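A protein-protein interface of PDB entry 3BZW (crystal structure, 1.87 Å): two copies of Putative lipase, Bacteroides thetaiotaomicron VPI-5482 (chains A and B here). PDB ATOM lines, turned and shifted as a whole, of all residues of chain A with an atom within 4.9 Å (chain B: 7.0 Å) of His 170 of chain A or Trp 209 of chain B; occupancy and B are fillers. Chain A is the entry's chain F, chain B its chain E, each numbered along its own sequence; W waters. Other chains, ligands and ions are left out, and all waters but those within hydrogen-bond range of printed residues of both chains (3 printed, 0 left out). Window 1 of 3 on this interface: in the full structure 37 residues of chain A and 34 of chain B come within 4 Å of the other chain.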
ATOM      1  N   PRO A 168       3.284   8.419 -10.729  1.00  0.00           N
ATOM      2  CA  PRO A 168       2.272   7.902  -9.801  1.00  0.00           C
ATOM      3  C   PRO A 168       2.650   6.521  -9.268  1.00  0.00           C
ATOM      4  O   PRO A 168       3.290   5.731  -9.964  1.00  0.00           O
ATOM      5  CB  PRO A 168       1.013   7.845 -10.660  1.00  0.00           C
ATOM      6  CG  PRO A 168       1.206   8.969 -11.613  1.00  0.00           C
ATOM      7  CD  PRO A 168       2.659   8.828 -11.998  1.00  0.00           C
ATOM      8  N   LEU A 169       2.238   6.240  -8.037  1.00  0.00           N
ATOM      9  CA  LEU A 169       2.531   4.970  -7.392  1.00  0.00           C
ATOM     10  C   LEU A 169       1.580   3.874  -7.839  1.00  0.00           C
ATOM     11  O   LEU A 169       0.484   4.144  -8.337  1.00  0.00           O
ATOM     12  CB  LEU A 169       2.396   5.097  -5.872  1.00  0.00           C
ATOM     13  CG  LEU A 169       3.225   6.112  -5.089  1.00  0.00           C
ATOM     14  CD1 LEU A 169       2.794   6.071  -3.626  1.00  0.00           C
ATOM     15  CD2 LEU A 169       4.704   5.793  -5.225  1.00  0.00           C
ATOM     16  N   HIS A 170       2.010   2.629  -7.652  1.00  0.00           N
ATOM     17  CA  HIS A 170       1.161   1.493  -7.968  1.00  0.00           C
ATOM     18  C   HIS A 170      -0.037   1.642  -7.036  1.00  0.00           C
ATOM     19  O   HIS A 170       0.081   2.243  -5.964  1.00  0.00           O
ATOM     20  CB  HIS A 170       1.914   0.192  -7.713  1.00  0.00           C
ATOM     21  CG  HIS A 170       2.776  -0.223  -8.863  1.00  0.00           C
ATOM     22  ND1 HIS A 170       2.360  -1.142  -9.804  1.00  0.00           N
ATOM     23  CD2 HIS A 170       3.996   0.202  -9.265  1.00  0.00           C
ATOM     24  CE1 HIS A 170       3.289  -1.263 -10.736  1.00  0.00           C
ATOM     25  NE2 HIS A 170       4.291  -0.458 -10.433  1.00  0.00           N
ATOM     26  N   ARG A 171      -1.180   1.106  -7.443  1.00  0.00           N
ATOM     27  CA  ARG A 171      -2.404   1.243  -6.665  1.00  0.00           C
ATOM     28  C   ARG A 171      -3.327   0.035  -6.777  1.00  0.00           C
ATOM     29  O   ARG A 171      -3.341  -0.663  -7.795  1.00  0.00           O
ATOM     30  CB  ARG A 171      -3.150   2.487  -7.155  1.00  0.00           C
ATOM     31  CG  ARG A 171      -3.225   2.576  -8.688  1.00  0.00           C
ATOM     32  CD  ARG A 171      -4.070   3.757  -9.145  1.00  0.00           C
ATOM     33  NE  ARG A 171      -5.470   3.585  -8.761  1.00  0.00           N
ATOM     34  CZ  ARG A 171      -6.336   4.583  -8.624  1.00  0.00           C
ATOM     35  NH1 ARG A 171      -5.949   5.840  -8.836  1.00  0.00           N
ATOM     36  NH2 ARG A 171      -7.591   4.326  -8.273  1.00  0.00           N
ATOM     37  N   SER A 172      -4.100  -0.199  -5.723  1.00  0.00           N
ATOM     38  CA  SER A 172      -5.050  -1.298  -5.700  1.00  0.00           C
ATOM     39  C   SER A 172      -6.438  -0.732  -5.406  1.00  0.00           C
ATOM     40  O   SER A 172      -6.669   0.469  -5.556  1.00  0.00           O
ATOM     41  CB  SER A 172      -4.653  -2.334  -4.647  1.00  0.00           C
ATOM     42  OG  SER A 172      -5.515  -3.465  -4.702  1.00  0.00           O
ATOM     43  N   GLU A 185      -5.539  -1.745  -9.990  1.00  0.00           N
ATOM     44  CA  GLU A 185      -4.853  -1.491 -11.254  1.00  0.00           C
ATOM     45  C   GLU A 185      -4.777  -2.622 -12.268  1.00  0.00           C
ATOM     46  O   GLU A 185      -4.106  -2.478 -13.286  1.00  0.00           O
ATOM     47  CB  GLU A 185      -3.437  -0.951 -11.004  1.00  0.00           C
ATOM     48  CG  GLU A 185      -2.489  -1.906 -10.308  1.00  0.00           C
ATOM     49  CD  GLU A 185      -1.087  -1.327 -10.189  1.00  0.00           C
ATOM     50  OE1 GLU A 185      -0.961  -0.088 -10.055  1.00  0.00           O
ATOM     51  OE2 GLU A 185      -0.115  -2.111 -10.220  1.00  0.00           O
ATOM     52  N   ASN A 217       7.133   5.436  -9.281  1.00  0.00           N
ATOM     53  CA  ASN A 217       6.331   4.239  -9.498  1.00  0.00           C
ATOM     54  C   ASN A 217       7.171   2.981  -9.296  1.00  0.00           C
ATOM     55  O   ASN A 217       6.708   1.988  -8.725  1.00  0.00           O
ATOM     56  CB  ASN A 217       5.754   4.269 -10.916  1.00  0.00           C
ATOM     57  CG  ASN A 217       4.943   3.033 -11.247  1.00  0.00           C
ATOM     58  OD1 ASN A 217       5.473   2.043 -11.759  1.00  0.00           O
ATOM     59  ND2 ASN A 217       3.645   3.082 -10.952  1.00  0.00           N
ATOM     60  N   MET A 222       7.106   0.024  -3.786  1.00  0.00           N
ATOM     61  CA  MET A 222       5.824  -0.201  -3.126  1.00  0.00           C
ATOM     62  C   MET A 222       4.726  -0.588  -4.110  1.00  0.00           C
ATOM     63  O   MET A 222       4.339   0.207  -4.962  1.00  0.00           O
ATOM     64  CB  MET A 222       5.413   1.057  -2.358  1.00  0.00           C
ATOM     65  CG  MET A 222       6.255   1.300  -1.103  1.00  0.00           C
ATOM     66  SD  MET A 222       6.124   3.094  -0.403  1.00  0.00           S
ATOM     67  CE  MET A 222       4.195   3.336  -0.512  1.00  0.00           C
ATOM     68  N   ASN A 223       4.224  -1.815  -3.984  1.00  0.00           N
ATOM     69  CA  ASN A 223       3.172  -2.303  -4.870  1.00  0.00           C
ATOM     70  C   ASN A 223       2.057  -2.970  -4.065  1.00  0.00           C
ATOM     71  O   ASN A 223       2.199  -4.113  -3.627  1.00  0.00           O
ATOM     72  CB  ASN A 223       3.756  -3.306  -5.865  1.00  0.00           C
ATOM     73  CG  ASN A 223       2.759  -3.719  -6.931  1.00  0.00           C
ATOM     74  OD1 ASN A 223       1.563  -3.433  -6.831  1.00  0.00           O
ATOM     75  ND2 ASN A 223       3.247  -4.403  -7.961  1.00  0.00           N
ATOM     76  N   PRO A 224       0.926  -2.272  -3.878  1.00  0.00           N
ATOM     77  CA  PRO A 224      -0.201  -2.820  -3.118  1.00  0.00           C
ATOM     78  C   PRO A 224      -0.859  -4.042  -3.752  1.00  0.00           C
ATOM     79  O   PRO A 224      -1.682  -4.707  -3.113  1.00  0.00           O
ATOM     80  CB  PRO A 224      -1.152  -1.631  -3.001  1.00  0.00           C
ATOM     81  CG  PRO A 224      -0.914  -0.897  -4.280  1.00  0.00           C
ATOM     82  CD  PRO A 224       0.597  -0.940  -4.419  1.00  0.00           C
ATOM     83  N   VAL A 226       0.588  -6.608  -4.264  1.00  0.00           N
ATOM     84  CA  VAL A 226       1.184  -7.716  -3.520  1.00  0.00           C
ATOM     85  C   VAL A 226       0.715  -7.428  -2.098  1.00  0.00           C
ATOM     86  O   VAL A 226       1.195  -6.500  -1.449  1.00  0.00           O
ATOM     87  CB  VAL A 226       2.729  -7.700  -3.582  1.00  0.00           C
ATOM     88  CG1 VAL A 226       3.290  -8.833  -2.735  1.00  0.00           C
ATOM     89  CG2 VAL A 226       3.194  -7.856  -5.027  1.00  0.00           C
ATOM     90  N   PHE A 233       0.142   0.781   3.094  1.00  0.00           N
ATOM     91  CA  PHE A 233      -1.077   1.468   2.684  1.00  0.00           C
ATOM     92  C   PHE A 233      -2.089   1.603   3.824  1.00  0.00           C
ATOM     93  O   PHE A 233      -2.016   0.886   4.820  1.00  0.00           O
ATOM     94  CB  PHE A 233      -1.648   0.768   1.446  1.00  0.00           C
ATOM     95  CG  PHE A 233      -0.777   0.936   0.222  1.00  0.00           C
ATOM     96  CD1 PHE A 233      -1.036   1.947  -0.701  1.00  0.00           C
ATOM     97  CD2 PHE A 233       0.350   0.140   0.042  1.00  0.00           C
ATOM     98  CE1 PHE A 233      -0.182   2.167  -1.785  1.00  0.00           C
ATOM     99  CE2 PHE A 233       1.214   0.352  -1.041  1.00  0.00           C
ATOM    100  CZ  PHE A 233       0.949   1.367  -1.953  1.00  0.00           C
ATOM    101  N   TRP B 110       3.773 -10.770 -20.273  1.00  0.00           N
ATOM    102  CA  TRP B 110       3.634 -10.370 -18.877  1.00  0.00           C
ATOM    103  C   TRP B 110       2.268 -10.732 -18.299  1.00  0.00           C
ATOM    104  O   TRP B 110       2.174 -11.223 -17.171  1.00  0.00           O
ATOM    105  CB  TRP B 110       3.840  -8.862 -18.730  1.00  0.00           C
ATOM    106  CG  TRP B 110       5.224  -8.385 -19.058  1.00  0.00           C
ATOM    107  CD1 TRP B 110       5.598  -7.603 -20.118  1.00  0.00           C
ATOM    108  CD2 TRP B 110       6.409  -8.608 -18.285  1.00  0.00           C
ATOM    109  NE1 TRP B 110       6.946  -7.322 -20.048  1.00  0.00           N
ATOM    110  CE2 TRP B 110       7.467  -7.926 -18.933  1.00  0.00           C
ATOM    111  CE3 TRP B 110       6.682  -9.316 -17.106  1.00  0.00           C
ATOM    112  CZ2 TRP B 110       8.778  -7.929 -18.437  1.00  0.00           C
ATOM    113  CZ3 TRP B 110       7.993  -9.319 -16.611  1.00  0.00           C
ATOM    114  CH2 TRP B 110       9.020  -8.629 -17.277  1.00  0.00           C
ATOM    115  N   PHE B 111       1.214 -10.488 -19.076  1.00  0.00           N
ATOM    116  CA  PHE B 111      -0.154 -10.757 -18.627  1.00  0.00           C
ATOM    117  C   PHE B 111      -1.018 -11.401 -19.697  1.00  0.00           C
ATOM    118  O   PHE B 111      -0.656 -11.455 -20.871  1.00  0.00           O
ATOM    119  CB  PHE B 111      -0.890  -9.454 -18.289  1.00  0.00           C
ATOM    120  CG  PHE B 111      -0.214  -8.587 -17.273  1.00  0.00           C
ATOM    121  CD1 PHE B 111      -0.486  -8.740 -15.918  1.00  0.00           C
ATOM    122  CD2 PHE B 111       0.639  -7.566 -17.678  1.00  0.00           C
ATOM    123  CE1 PHE B 111       0.076  -7.879 -14.977  1.00  0.00           C
ATOM    124  CE2 PHE B 111       1.207  -6.702 -16.747  1.00  0.00           C
ATOM    125  CZ  PHE B 111       0.925  -6.856 -15.395  1.00  0.00           C
ATOM    126  N   ARG B 134      -6.421  -7.633 -16.442  1.00  0.00           N
ATOM    127  CA  ARG B 134      -5.215  -8.388 -16.751  1.00  0.00           C
ATOM    128  C   ARG B 134      -4.807  -9.243 -15.562  1.00  0.00           C
ATOM    129  O   ARG B 134      -5.079  -8.899 -14.409  1.00  0.00           O
ATOM    130  CB  ARG B 134      -4.072  -7.444 -17.140  1.00  0.00           C
ATOM    131  CG  ARG B 134      -3.703  -6.429 -16.078  1.00  0.00           C
ATOM    132  CD  ARG B 134      -2.594  -5.506 -16.576  1.00  0.00           C
ATOM    133  NE  ARG B 134      -2.289  -4.455 -15.611  1.00  0.00           N
ATOM    134  CZ  ARG B 134      -1.545  -3.389 -15.884  1.00  0.00           C
ATOM    135  NH1 ARG B 134      -1.027  -3.239 -17.096  1.00  0.00           N
ATOM    136  NH2 ARG B 134      -1.338  -2.465 -14.954  1.00  0.00           N
ATOM    137  N   PRO B 136      -1.352 -11.527 -14.183  1.00  0.00           N
ATOM    138  CA  PRO B 136       0.056 -11.855 -14.425  1.00  0.00           C
ATOM    139  C   PRO B 136       0.205 -13.315 -14.833  1.00  0.00           C
ATOM    140  O   PRO B 136      -0.494 -14.179 -14.307  1.00  0.00           O
ATOM    141  CB  PRO B 136       0.716 -11.592 -13.070  1.00  0.00           C
ATOM    142  CG  PRO B 136      -0.197 -10.598 -12.411  1.00  0.00           C
ATOM    143  CD  PRO B 136      -1.560 -11.104 -12.787  1.00  0.00           C
ATOM    144  N   VAL B 137       1.102 -13.592 -15.774  1.00  0.00           N
ATOM    145  CA  VAL B 137       1.330 -14.971 -16.187  1.00  0.00           C
ATOM    146  C   VAL B 137       2.315 -15.563 -15.184  1.00  0.00           C
ATOM    147  O   VAL B 137       3.445 -15.091 -15.063  1.00  0.00           O
ATOM    148  CB  VAL B 137       1.932 -15.044 -17.602  1.00  0.00           C
ATOM    149  CG1 VAL B 137       2.228 -16.492 -17.964  1.00  0.00           C
ATOM    150  CG2 VAL B 137       0.964 -14.436 -18.610  1.00  0.00           C
ATOM    151  N   MET B 138       1.878 -16.580 -14.447  1.00  0.00           N
ATOM    152  CA  MET B 138       2.728 -17.217 -13.445  1.00  0.00           C
ATOM    153  C   MET B 138       3.168 -18.602 -13.911  1.00  0.00           C
ATOM    154  O   MET B 138       2.598 -19.612 -13.510  1.00  0.00           O
ATOM    155  CB  MET B 138       1.977 -17.336 -12.112  1.00  0.00           C
ATOM    156  CG  MET B 138       1.490 -16.008 -11.529  1.00  0.00           C
ATOM    157  SD  MET B 138       2.915 -14.820 -10.938  1.00  0.00           S
ATOM    158  CE  MET B 138       3.098 -15.462  -9.122  1.00  0.00           C
ATOM    159  N   ARG B 144       9.404 -13.872 -18.801  1.00  0.00           N
ATOM    160  CA  ARG B 144       8.534 -12.935 -18.104  1.00  0.00           C
ATOM    161  C   ARG B 144       7.748 -13.671 -17.024  1.00  0.00           C
ATOM    162  O   ARG B 144       7.471 -13.123 -15.960  1.00  0.00           O
ATOM    163  CB  ARG B 144       7.599 -12.248 -19.107  1.00  0.00           C
ATOM    164  CG  ARG B 144       8.318 -11.195 -19.951  1.00  0.00           C
ATOM    165  CD  ARG B 144       7.527 -10.759 -21.173  1.00  0.00           C
ATOM    166  NE  ARG B 144       8.087  -9.547 -21.777  1.00  0.00           N
ATOM    167  CZ  ARG B 144       7.728  -9.066 -22.965  1.00  0.00           C
ATOM    168  NH1 ARG B 144       6.814  -9.698 -23.688  1.00  0.00           N
ATOM    169  NH2 ARG B 144       8.263  -7.938 -23.421  1.00  0.00           N
ATOM    170  N   ILE B 147      10.073 -14.066 -14.149  1.00  0.00           N
ATOM    171  CA  ILE B 147      10.268 -12.785 -13.486  1.00  0.00           C
ATOM    172  C   ILE B 147       9.034 -12.482 -12.627  1.00  0.00           C
ATOM    173  O   ILE B 147       9.153 -12.035 -11.482  1.00  0.00           O
ATOM    174  CB  ILE B 147      10.495 -11.666 -14.520  1.00  0.00           C
ATOM    175  CG1 ILE B 147      11.812 -11.923 -15.269  1.00  0.00           C
ATOM    176  CG2 ILE B 147      10.508 -10.311 -13.831  1.00  0.00           C
ATOM    177  CD1 ILE B 147      12.100 -10.940 -16.401  1.00  0.00           C
ATOM    178  N   ASN B 148       7.850 -12.737 -13.174  1.00  0.00           N
ATOM    179  CA  ASN B 148       6.619 -12.497 -12.427  1.00  0.00           C
ATOM    180  C   ASN B 148       6.624 -13.298 -11.126  1.00  0.00           C
ATOM    181  O   ASN B 148       6.351 -12.765 -10.053  1.00  0.00           O
ATOM    182  CB  ASN B 148       5.383 -12.889 -13.251  1.00  0.00           C
ATOM    183  CG  ASN B 148       5.089 -11.911 -14.376  1.00  0.00           C
ATOM    184  OD1 ASN B 148       5.574 -10.778 -14.376  1.00  0.00           O
ATOM    185  ND2 ASN B 148       4.276 -12.342 -15.335  1.00  0.00           N
ATOM    186  N   ILE B 149       6.946 -14.582 -11.236  1.00  0.00           N
ATOM    187  CA  ILE B 149       6.986 -15.477 -10.086  1.00  0.00           C
ATOM    188  C   ILE B 149       8.066 -15.050  -9.097  1.00  0.00           C
ATOM    189  O   ILE B 149       7.836 -15.007  -7.884  1.00  0.00           O
ATOM    190  CB  ILE B 149       7.265 -16.938 -10.538  1.00  0.00           C
ATOM    191  CG1 ILE B 149       6.087 -17.453 -11.375  1.00  0.00           C
ATOM    192  CG2 ILE B 149       7.518 -17.823  -9.322  1.00  0.00           C
ATOM    193  CD1 ILE B 149       6.308 -18.823 -12.009  1.00  0.00           C
ATOM    194  N   ILE B 151       9.698 -12.004  -8.666  1.00  0.00           N
ATOM    195  CA  ILE B 151       9.472 -10.744  -7.975  1.00  0.00           C
ATOM    196  C   ILE B 151       8.337 -10.904  -6.962  1.00  0.00           C
ATOM    197  O   ILE B 151       8.403 -10.357  -5.862  1.00  0.00           O
ATOM    198  CB  ILE B 151       9.189  -9.611  -8.985  1.00  0.00           C
ATOM    199  CG1 ILE B 151      10.446  -9.382  -9.837  1.00  0.00           C
ATOM    200  CG2 ILE B 151       8.815  -8.323  -8.251  1.00  0.00           C
ATOM    201  CD1 ILE B 151      10.336  -8.274 -10.861  1.00  0.00           C
ATOM    202  N   THR B 152       7.313 -11.678  -7.318  1.00  0.00           N
ATOM    203  CA  THR B 152       6.209 -11.905  -6.392  1.00  0.00           C
ATOM    204  C   THR B 152       6.736 -12.537  -5.101  1.00  0.00           C
ATOM    205  O   THR B 152       6.434 -12.068  -3.999  1.00  0.00           O
ATOM    206  CB  THR B 152       5.131 -12.832  -7.003  1.00  0.00           C
ATOM    207  OG1 THR B 152       4.467 -12.151  -8.075  1.00  0.00           O
ATOM    208  CG2 THR B 152       4.097 -13.224  -5.947  1.00  0.00           C
ATOM    209  N   LYS B 155       8.836 -10.085  -3.004  1.00  0.00           N
ATOM    210  CA  LYS B 155       8.007  -9.121  -2.283  1.00  0.00           C
ATOM    211  C   LYS B 155       7.196  -9.752  -1.153  1.00  0.00           C
ATOM    212  O   LYS B 155       6.946  -9.108  -0.136  1.00  0.00           O
ATOM    213  CB  LYS B 155       7.070  -8.383  -3.253  1.00  0.00           C
ATOM    214  CG  LYS B 155       7.767  -7.289  -4.065  1.00  0.00           C
ATOM    215  CD  LYS B 155       6.804  -6.571  -5.005  1.00  0.00           C
ATOM    216  CE  LYS B 155       7.504  -5.432  -5.752  1.00  0.00           C
ATOM    217  NZ  LYS B 155       7.923  -4.325  -4.849  1.00  0.00           N
ATOM    218  N   LEU B 165      16.990  -4.918  -8.778  1.00  0.00           N
ATOM    219  CA  LEU B 165      17.323  -5.829  -9.868  1.00  0.00           C
ATOM    220  C   LEU B 165      18.468  -5.248 -10.684  1.00  0.00           C
ATOM    221  O   LEU B 165      18.538  -4.033 -10.882  1.00  0.00           O
ATOM    222  CB  LEU B 165      16.119  -6.034 -10.795  1.00  0.00           C
ATOM    223  CG  LEU B 165      14.772  -6.455 -10.199  1.00  0.00           C
ATOM    224  CD1 LEU B 165      13.768  -6.663 -11.336  1.00  0.00           C
ATOM    225  CD2 LEU B 165      14.924  -7.733  -9.397  1.00  0.00           C
ATOM    226  N   GLU B 204      11.890  -3.456 -17.899  1.00  0.00           N
ATOM    227  CA  GLU B 204      10.438  -3.285 -17.933  1.00  0.00           C
ATOM    228  C   GLU B 204       9.786  -3.711 -16.622  1.00  0.00           C
ATOM    229  O   GLU B 204       8.751  -3.172 -16.237  1.00  0.00           O
ATOM    230  CB  GLU B 204       9.840  -4.099 -19.087  1.00  0.00           C
ATOM    231  CG  GLU B 204      10.461  -3.772 -20.436  1.00  0.00           C
ATOM    232  CD  GLU B 204       9.986  -4.684 -21.549  1.00  0.00           C
ATOM    233  OE1 GLU B 204       9.511  -5.800 -21.254  1.00  0.00           O
ATOM    234  OE2 GLU B 204      10.109  -4.289 -22.725  1.00  0.00           O
ATOM    235  N   ALA B 205      10.388  -4.676 -15.934  1.00  0.00           N
ATOM    236  CA  ALA B 205       9.825  -5.154 -14.673  1.00  0.00           C
ATOM    237  C   ALA B 205       9.754  -4.047 -13.624  1.00  0.00           C
ATOM    238  O   ALA B 205       8.966  -4.126 -12.677  1.00  0.00           O
ATOM    239  CB  ALA B 205      10.648  -6.321 -14.145  1.00  0.00           C
ATOM    240  N   GLY B 206      10.577  -3.016 -13.795  1.00  0.00           N
ATOM    241  CA  GLY B 206      10.589  -1.917 -12.844  1.00  0.00           C
ATOM    242  C   GLY B 206       9.218  -1.302 -12.635  1.00  0.00           C
ATOM    243  O   GLY B 206       8.728  -1.202 -11.506  1.00  0.00           O
ATOM    244  N   ASN B 207       8.588  -0.895 -13.728  1.00  0.00           N
ATOM    245  CA  ASN B 207       7.268  -0.282 -13.656  1.00  0.00           C
ATOM    246  C   ASN B 207       6.166  -1.318 -13.519  1.00  0.00           C
ATOM    247  O   ASN B 207       5.150  -1.066 -12.879  1.00  0.00           O
ATOM    248  CB  ASN B 207       7.011   0.567 -14.902  1.00  0.00           C
ATOM    249  CG  ASN B 207       7.781   1.870 -14.884  1.00  0.00           C
ATOM    250  OD1 ASN B 207       8.466   2.216 -15.849  1.00  0.00           O
ATOM    251  ND2 ASN B 207       7.664   2.609 -13.785  1.00  0.00           N
ATOM    252  N   ILE B 208       6.365  -2.489 -14.109  1.00  0.00           N
ATOM    253  CA  ILE B 208       5.339  -3.521 -14.033  1.00  0.00           C
ATOM    254  C   ILE B 208       5.104  -4.002 -12.608  1.00  0.00           C
ATOM    255  O   ILE B 208       3.957  -4.174 -12.195  1.00  0.00           O
ATOM    256  CB  ILE B 208       5.687  -4.733 -14.912  1.00  0.00           C
ATOM    257  CG1 ILE B 208       5.718  -4.303 -16.381  1.00  0.00           C
ATOM    258  CG2 ILE B 208       4.645  -5.835 -14.721  1.00  0.00           C
ATOM    259  CD1 ILE B 208       6.232  -5.383 -17.320  1.00  0.00           C
ATOM    260  N   TRP B 209       6.184  -4.208 -11.859  1.00  0.00           N
ATOM    261  CA  TRP B 209       6.074  -4.694 -10.488  1.00  0.00           C
ATOM    262  C   TRP B 209       6.323  -3.661  -9.402  1.00  0.00           C
ATOM    263  O   TRP B 209       5.981  -3.891  -8.243  1.00  0.00           O
ATOM    264  CB  TRP B 209       7.024  -5.878 -10.274  1.00  0.00           C
ATOM    265  CG  TRP B 209       6.516  -7.121 -10.911  1.00  0.00           C
ATOM    266  CD1 TRP B 209       6.873  -7.633 -12.124  1.00  0.00           C
ATOM    267  CD2 TRP B 209       5.471  -7.959 -10.413  1.00  0.00           C
ATOM    268  NE1 TRP B 209       6.111  -8.741 -12.415  1.00  0.00           N
ATOM    269  CE2 TRP B 209       5.240  -8.963 -11.380  1.00  0.00           C
ATOM    270  CE3 TRP B 209       4.703  -7.958  -9.241  1.00  0.00           C
ATOM    271  CZ2 TRP B 209       4.273  -9.957 -11.212  1.00  0.00           C
ATOM    272  CZ3 TRP B 209       3.738  -8.947  -9.070  1.00  0.00           C
ATOM    273  CH2 TRP B 209       3.533  -9.934 -10.054  1.00  0.00           C
ATOM    274  N   GLY B 210       6.908  -2.528  -9.773  1.00  0.00           N
ATOM    275  CA  GLY B 210       7.200  -1.499  -8.790  1.00  0.00           C
ATOM    276  C   GLY B 210       8.456  -1.892  -8.040  1.00  0.00           C
ATOM    277  O   GLY B 210       8.417  -2.200  -6.845  1.00  0.00           O
ATOM    278  N   ILE B 211       9.581  -1.881  -8.741  1.00  0.00           N
ATOM    279  CA  ILE B 211      10.845  -2.272  -8.126  1.00  0.00           C
ATOM    280  C   ILE B 211      11.991  -1.540  -8.816  1.00  0.00           C
ATOM    281  O   ILE B 211      11.966  -1.338 -10.031  1.00  0.00           O
ATOM    282  CB  ILE B 211      11.021  -3.820  -8.237  1.00  0.00           C
ATOM    283  CG1 ILE B 211      12.265  -4.285  -7.483  1.00  0.00           C
ATOM    284  CG2 ILE B 211      11.092  -4.235  -9.705  1.00  0.00           C
ATOM    285  CD1 ILE B 211      12.308  -5.803  -7.297  1.00  0.00           C
HETATM  286  O   HOH W   1      -2.266  -5.328 -12.896  1.00  0.00           O
HETATM  287  O   HOH W   2       3.599   1.421 -13.942  1.00  0.00           O
HETATM  288  O   HOH W   3       2.030  -5.765 -10.724  1.00  0.00           O
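The backbone NH (N) of Gly 210 of chain B sits at hydrogen-bond distance from a ring nitrogen (NE2) of His 170 of chain A (3.4 Å). NH2 of Arg 134 of chain B sits at hydrogen-bond distance from O of Glu 185 of chain A, at 3.2 Å. ND2 of Asn 223 of chain A sits at hydrogen-bond distance from O of Trp 209 of chain B. The backbone carbonyl oxygen (O) of Asn 207 of chain B sits at hydrogen-bond distance from a ring nitrogen (NE2) of His 170 of chain A (2.7 Å). The side-chain amide nitrogen (ND2) of Asn 207 of chain B is in hydrogen-bond range of the side-chain amide oxygen (OD1) of Asn 217 of chain A.
The backbone NH (N) of Arg 171 of chain A lies within hydrogen-bond range of the side-chain carboxylate (OE1) of Glu 185 of chain A (2.9 Å). NE2 of His 170 of chain A lies within hydrogen-bond range of OD1 of Asn 217 of chain A (3.1 Å). O of Gly 210 of chain B is in hydrogen-bond range of NZ of Lys 155 of chain B (3.0 Å). OD1 of Asn 148 of chain B is in hydrogen-bond range of NE1 of Trp 209 of chain B (2.9 Å). ND1 of His 170 of chain A sits at hydrogen-bond distance from OE2 of Glu 185 of chain A, at 2.7 Å. The side-chain amide nitrogen (ND2) of Asn 217 of chain A sits at hydrogen-bond distance from the backbone carbonyl oxygen (O) of Pro 168 of chain A, 2.8 Å away.
His 170 of chain A touches Ile 208 of chain B. His 170 of chain A touches Trp 209 of chain B. Asn 217 of chain A touches Gly 210 of chain B (O to CA, 3.5 Å). Val 226 of chain A touches Lys 155 of chain B.
His 170 of chain A touches just these residues of chain B: Asn 207 (2.7 Å), Ile 208 (3.3 Å), Trp 209 (3.9 Å) and Gly 210 (3.4 Å). Printed residues of chain B within 4 Å of Glu 185 of chain A: Arg 134. Printed residues of chain B within 4 Å of Asn 217 of chain A: Asn 207 and Gly 210. Of the printed residues of chain B, Val 226 of chain A touches Lys 155 (3.8 Å). Of the printed residues of chain A, Gly 210 of chain B touches His 170 and Asn 217. Ala 205 of chain B touches none of the printed residues of chain A. The nearest residue of chain A that does not touch Trp 209 of chain B is Val 226 of chain A (4.2 Å). The nearest printed residue of chain B that does not touch Val 226 of chain A is Trp 209 of chain B (4.2 Å).
Printed residues of chain B that touch a printed residue of chain A: Arg 134, Lys 155, Asn 207, Ile 208, Trp 209 and Gly 210. Along chain B the printed residues that touch a printed residue of chain A span positions 134 to 210.
No position is printed for both chains. Of the 9 pairs that touch across the chains among the printed residues, none has its exchanged pair printed and touching as well.
Water W1 bridges NE of Arg 134 of chain B (2.9 Å) and O of Glu 185 of chain A (3.4 Å). Water W3 bridges the backbone carbonyl oxygen (O) of Ile 208 of chain B and the side-chain amide nitrogen (ND2) of Asn 223 of chain A. Water W2 lies within hydrogen-bond range of the side-chain amide oxygen of Asn 217 of chain A (2.9 Å) and the backbone carbonyl oxygen of Asn 207 of chain B (3.1 Å).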
